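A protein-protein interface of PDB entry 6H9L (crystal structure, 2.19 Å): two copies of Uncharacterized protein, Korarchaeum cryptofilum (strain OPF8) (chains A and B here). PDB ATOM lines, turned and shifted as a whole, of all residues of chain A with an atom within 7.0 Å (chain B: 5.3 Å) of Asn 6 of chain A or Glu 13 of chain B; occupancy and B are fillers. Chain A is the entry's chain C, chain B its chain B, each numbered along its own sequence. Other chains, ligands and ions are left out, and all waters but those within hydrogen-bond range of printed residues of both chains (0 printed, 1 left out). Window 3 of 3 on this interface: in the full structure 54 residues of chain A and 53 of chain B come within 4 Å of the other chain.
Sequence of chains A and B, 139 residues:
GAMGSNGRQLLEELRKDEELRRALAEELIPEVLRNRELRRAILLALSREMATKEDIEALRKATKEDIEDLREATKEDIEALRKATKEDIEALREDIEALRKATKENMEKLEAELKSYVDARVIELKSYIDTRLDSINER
O of Asn 6 of chain B sits at hydrogen-bond distance from ND2 of Asn 6 of chain A (2.9 Å).
The backbone NH (N) of Asn 6 of chain A lies close to the side-chain carboxylate (OE2) of Glu 13 of chain B, at 3.5 Å.
The side-chain carboxylate of Glu 13 of chain B lies within hydrogen-bond range of the backbone NH of Gly 7 of chain A (3.1 Å).
OD1 of Asp 17 of chain B is in hydrogen-bond range of N of Leu 20 of chain B, 3.4 Å away.
Gly 7 of chain A touches Leu 10 of chain B.
Gly 7 of chain A touches Leu 20 of chain B.
CD2 of Leu 10 of chain A touches CD2 of Leu 10 of chain B, 3.4 Å away.
Asn 6 of chain A touches just these residues of chain B: Asn 6 and Glu 13.
Printed residues of chain A within 4 Å of Glu 13 of chain B: Asn 6 (3.3 Å) and Gly 7 (3.1 Å).
Of the printed residues of chain B, Leu 10 of chain A touches Leu 10.
Of the printed residues of chain A, Leu 20 of chain B touches Gly 7 (3.7 Å).
Of the printed residues of chain A, Asn 6 of chain B touches Asn 6 (2.9 Å).
Gln 9 of chain A touches none of the printed residues of chain B.
Gly 7 of chain B touches none of the printed residues of chain A.
The nearest residue of chain A that does not touch Glu 13 of chain B is Arg 8 of chain A (4.7 Å).
Of the 12 printed residues of chain B, 4 touch a printed residue of chain A.
Hydrophobic or aromatic side chains of chain B that line the printed part of chain A: Leu 10 and Leu 20.
Of the 6 printed residues of chain A, 3 touch a printed residue of chain B.
Hydrophobic or aromatic side chains of chain A that line the printed part of chain B: Leu 10.
Among the printed residues, 6 pairs touch across the chains.
Asn 6 of chain B touches its own counterpart, Asn 6 of chain A.
Gly 7 of chain A touches Leu 10 of chain B, but with the chains exchanged Leu 10 of chain A does not touch Gly 7 of chain B (8.0 Å).
Leu 10 of chain A touches its own counterpart, Leu 10 of chain B.
Positions printed for both chains: 6, 7, 9, 10 and 11.
Of the 6 pairs that touch across the chains among the printed residues, 2 have their exchanged pair printed and touching as well.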
ATOM      1  N   ASN A   6      21.682   9.445  26.595  1.00  0.00           N
ATOM      2  CA  ASN A   6      22.907   9.843  25.830  1.00  0.00           C
ATOM      3  C   ASN A   6      24.025  10.296  26.773  1.00  0.00           C
ATOM      4  O   ASN A   6      25.168   9.842  26.668  1.00  0.00           O
ATOM      5  CB  ASN A   6      22.589  10.964  24.823  1.00  0.00           C
ATOM      6  CG  ASN A   6      23.440  10.886  23.561  1.00  0.00           C
ATOM      7  OD1 ASN A   6      23.677   9.808  23.005  1.00  0.00           O
ATOM      8  ND2 ASN A   6      23.903  12.043  23.098  1.00  0.00           N
ATOM      9  N   GLY A   7      23.679  11.202  27.686  1.00  0.00           N
ATOM     10  CA  GLY A   7      24.598  11.669  28.723  1.00  0.00           C
ATOM     11  C   GLY A   7      24.903  10.612  29.774  1.00  0.00           C
ATOM     12  O   GLY A   7      26.005  10.585  30.331  1.00  0.00           O
ATOM     13  N   ARG A   8      23.927   9.744  30.049  1.00  0.00           N
ATOM     14  CA  ARG A   8      24.110   8.639  30.990  1.00  0.00           C
ATOM     15  C   ARG A   8      25.153   7.661  30.455  1.00  0.00           C
ATOM     16  O   ARG A   8      26.027   7.201  31.196  1.00  0.00           O
ATOM     17  CB  ARG A   8      22.781   7.918  31.231  1.00  0.00           C
ATOM     18  N   GLN A   9      25.055   7.361  29.163  1.00  0.00           N
ATOM     19  CA  GLN A   9      26.056   6.549  28.467  1.00  0.00           C
ATOM     20  C   GLN A   9      27.436   7.213  28.485  1.00  0.00           C
ATOM     21  O   GLN A   9      28.444   6.561  28.770  1.00  0.00           O
ATOM     22  CB  GLN A   9      25.630   6.267  27.020  1.00  0.00           C
ATOM     23  CG  GLN A   9      24.463   5.299  26.929  1.00  0.00           C
ATOM     24  CD  GLN A   9      23.783   5.323  25.570  1.00  0.00           C
ATOM     25  OE1 GLN A   9      22.756   5.966  25.415  1.00  0.00           O
ATOM     26  NE2 GLN A   9      24.359   4.639  24.575  1.00  0.00           N
ATOM     27  N   LEU A  10      27.465   8.512  28.191  1.00  0.00           N
ATOM     28  CA  LEU A  10      28.708   9.285  28.169  1.00  0.00           C
ATOM     29  C   LEU A  10      29.411   9.221  29.518  1.00  0.00           C
ATOM     30  O   LEU A  10      30.613   8.967  29.592  1.00  0.00           O
ATOM     31  CB  LEU A  10      28.429  10.744  27.790  1.00  0.00           C
ATOM     32  CG  LEU A  10      29.626  11.707  27.749  1.00  0.00           C
ATOM     33  CD1 LEU A  10      30.721  11.212  26.817  1.00  0.00           C
ATOM     34  CD2 LEU A  10      29.163  13.095  27.336  1.00  0.00           C
ATOM     35  N   LEU A  11      28.651   9.461  30.581  1.00  0.00           N
ATOM     36  CA  LEU A  11      29.179   9.374  31.936  1.00  0.00           C
ATOM     37  C   LEU A  11      29.792   8.012  32.214  1.00  0.00           C
ATOM     38  O   LEU A  11      30.865   7.932  32.806  1.00  0.00           O
ATOM     39  CB  LEU A  11      28.085   9.707  32.940  1.00  0.00           C
ATOM     40  CG  LEU A  11      28.463   9.775  34.437  1.00  0.00           C
ATOM     41  CD1 LEU A  11      29.096  11.128  34.716  1.00  0.00           C
ATOM     42  CD2 LEU A  11      27.274   9.556  35.368  1.00  0.00           C
ATOM     43  N   ASN B   6      24.018  14.086  17.998  1.00  0.00           N
ATOM     44  CA  ASN B   6      24.380  13.416  19.244  1.00  0.00           C
ATOM     45  C   ASN B   6      24.769  14.436  20.317  1.00  0.00           C
ATOM     46  O   ASN B   6      24.294  14.377  21.455  1.00  0.00           O
ATOM     47  CB  ASN B   6      25.546  12.446  19.011  1.00  0.00           C
ATOM     48  CG  ASN B   6      25.507  11.246  19.944  1.00  0.00           C
ATOM     49  OD1 ASN B   6      24.450  10.648  20.184  1.00  0.00           O
ATOM     50  ND2 ASN B   6      26.667  10.885  20.476  1.00  0.00           N
ATOM     51  N   GLY B   7      25.637  15.370  19.935  1.00  0.00           N
ATOM     52  CA  GLY B   7      26.047  16.469  20.808  1.00  0.00           C
ATOM     53  C   GLY B   7      24.946  17.486  21.055  1.00  0.00           C
ATOM     54  O   GLY B   7      24.883  18.097  22.125  1.00  0.00           O
ATOM     55  N   GLN B   9      21.723  16.769  21.211  1.00  0.00           N
ATOM     56  CA  GLN B   9      20.920  16.089  22.233  1.00  0.00           C
ATOM     57  C   GLN B   9      21.562  16.200  23.611  1.00  0.00           C
ATOM     58  O   GLN B   9      20.887  16.508  24.599  1.00  0.00           O
ATOM     59  CB  GLN B   9      20.708  14.611  21.868  1.00  0.00           C
ATOM     60  CG  GLN B   9      19.766  14.424  20.689  1.00  0.00           C
ATOM     61  CD  GLN B   9      19.898  13.067  20.024  1.00  0.00           C
ATOM     62  OE1 GLN B   9      20.702  12.219  20.427  1.00  0.00           O
ATOM     63  NE2 GLN B   9      19.101  12.859  18.990  1.00  0.00           N
ATOM     64  N   LEU B  10      22.871  15.955  23.666  1.00  0.00           N
ATOM     65  CA  LEU B  10      23.629  16.028  24.914  1.00  0.00           C
ATOM     66  C   LEU B  10      23.512  17.411  25.545  1.00  0.00           C
ATOM     67  O   LEU B  10      23.240  17.530  26.743  1.00  0.00           O
ATOM     68  CB  LEU B  10      25.101  15.683  24.667  1.00  0.00           C
ATOM     69  CG  LEU B  10      26.052  15.735  25.868  1.00  0.00           C
ATOM     70  CD1 LEU B  10      25.580  14.848  27.010  1.00  0.00           C
ATOM     71  CD2 LEU B  10      27.457  15.343  25.434  1.00  0.00           C
ATOM     72  N   LEU B  11      23.717  18.445  24.729  1.00  0.00           N
ATOM     73  CA  LEU B  11      23.558  19.833  25.169  1.00  0.00           C
ATOM     74  C   LEU B  11      22.184  20.069  25.785  1.00  0.00           C
ATOM     75  O   LEU B  11      22.073  20.699  26.836  1.00  0.00           O
ATOM     76  CB  LEU B  11      23.785  20.824  24.007  1.00  0.00           C
ATOM     77  CG  LEU B  11      25.222  21.203  23.669  1.00  0.00           C
ATOM     78  CD1 LEU B  11      25.262  22.167  22.491  1.00  0.00           C
ATOM     79  CD2 LEU B  11      25.951  21.798  24.863  1.00  0.00           C
ATOM     80  N   GLU B  12      21.150  19.545  25.132  1.00  0.00           N
ATOM     81  CA  GLU B  12      19.774  19.672  25.617  1.00  0.00           C
ATOM     82  C   GLU B  12      19.591  19.031  26.997  1.00  0.00           C
ATOM     83  O   GLU B  12      19.034  19.654  27.908  1.00  0.00           O
ATOM     84  CB  GLU B  12      18.795  19.054  24.614  1.00  0.00           C
ATOM     85  N   GLU B  13      20.078  17.798  27.150  1.00  0.00           N
ATOM     86  CA  GLU B  13      19.984  17.076  28.430  1.00  0.00           C
ATOM     87  C   GLU B  13      20.719  17.834  29.550  1.00  0.00           C
ATOM     88  O   GLU B  13      20.244  17.898  30.690  1.00  0.00           O
ATOM     89  CB  GLU B  13      20.541  15.644  28.315  1.00  0.00           C
ATOM     90  CG  GLU B  13      20.045  14.823  27.127  1.00  0.00           C
ATOM     91  CD  GLU B  13      20.516  13.374  27.167  1.00  0.00           C
ATOM     92  OE1 GLU B  13      21.267  13.038  28.098  1.00  0.00           O
ATOM     93  OE2 GLU B  13      20.149  12.565  26.279  1.00  0.00           O
ATOM     94  N   LEU B  14      21.874  18.406  29.219  1.00  0.00           N
ATOM     95  CA  LEU B  14      22.671  19.161  30.190  1.00  0.00           C
ATOM     96  C   LEU B  14      21.963  20.424  30.681  1.00  0.00           C
ATOM     97  O   LEU B  14      22.056  20.760  31.863  1.00  0.00           O
ATOM     98  CB  LEU B  14      24.035  19.525  29.600  1.00  0.00           C
ATOM     99  CG  LEU B  14      24.989  18.347  29.408  1.00  0.00           C
ATOM    100  CD1 LEU B  14      26.094  18.702  28.425  1.00  0.00           C
ATOM    101  CD2 LEU B  14      25.584  17.912  30.737  1.00  0.00           C
ATOM    102  N   ARG B  15      21.270  21.122  29.782  1.00  0.00           N
ATOM    103  CA  ARG B  15      20.447  22.275  30.174  1.00  0.00           C
ATOM    104  C   ARG B  15      19.376  21.860  31.183  1.00  0.00           C
ATOM    105  O   ARG B  15      19.134  22.565  32.163  1.00  0.00           O
ATOM    106  CB  ARG B  15      19.768  22.934  28.962  1.00  0.00           C
ATOM    107  CG  ARG B  15      20.538  24.076  28.312  1.00  0.00           C
ATOM    108  CD  ARG B  15      21.626  23.562  27.410  1.00  0.00           C
ATOM    109  NE  ARG B  15      22.526  24.603  26.898  1.00  0.00           N
ATOM    110  CZ  ARG B  15      22.475  25.156  25.683  1.00  0.00           C
ATOM    111  NH1 ARG B  15      21.549  24.812  24.792  1.00  0.00           N
ATOM    112  NH2 ARG B  15      23.372  26.085  25.353  1.00  0.00           N
ATOM    113  N   LYS B  16      18.756  20.709  30.937  1.00  0.00           N
ATOM    114  CA  LYS B  16      17.660  20.211  31.769  1.00  0.00           C
ATOM    115  C   LYS B  16      18.127  19.605  33.098  1.00  0.00           C
ATOM    116  O   LYS B  16      17.528  19.871  34.140  1.00  0.00           O
ATOM    117  CB  LYS B  16      16.831  19.178  30.995  1.00  0.00           C
ATOM    118  N   ASP B  17      19.192  18.802  33.056  1.00  0.00           N
ATOM    119  CA  ASP B  17      19.618  17.982  34.198  1.00  0.00           C
ATOM    120  C   ASP B  17      20.919  18.503  34.821  1.00  0.00           C
ATOM    121  O   ASP B  17      22.006  18.286  34.289  1.00  0.00           O
ATOM    122  CB  ASP B  17      19.791  16.524  33.743  1.00  0.00           C
ATOM    123  CG  ASP B  17      19.948  15.544  34.905  1.00  0.00           C
ATOM    124  OD1 ASP B  17      20.100  15.976  36.067  1.00  0.00           O
ATOM    125  OD2 ASP B  17      19.924  14.321  34.646  1.00  0.00           O
ATOM    126  N   LEU B  20      23.463  15.785  35.921  1.00  0.00           N
ATOM    127  CA  LEU B  20      24.245  15.292  34.789  1.00  0.00           C
ATOM    128  C   LEU B  20      25.410  16.239  34.503  1.00  0.00           C
ATOM    129  O   LEU B  20      26.550  15.804  34.310  1.00  0.00           O
ATOM    130  CB  LEU B  20      23.353  15.150  33.550  1.00  0.00           C
ATOM    131  CG  LEU B  20      24.025  14.736  32.236  1.00  0.00           C
ATOM    132  CD1 LEU B  20      24.710  13.383  32.362  1.00  0.00           C
ATOM    133  CD2 LEU B  20      23.007  14.720  31.106  1.00  0.00           C
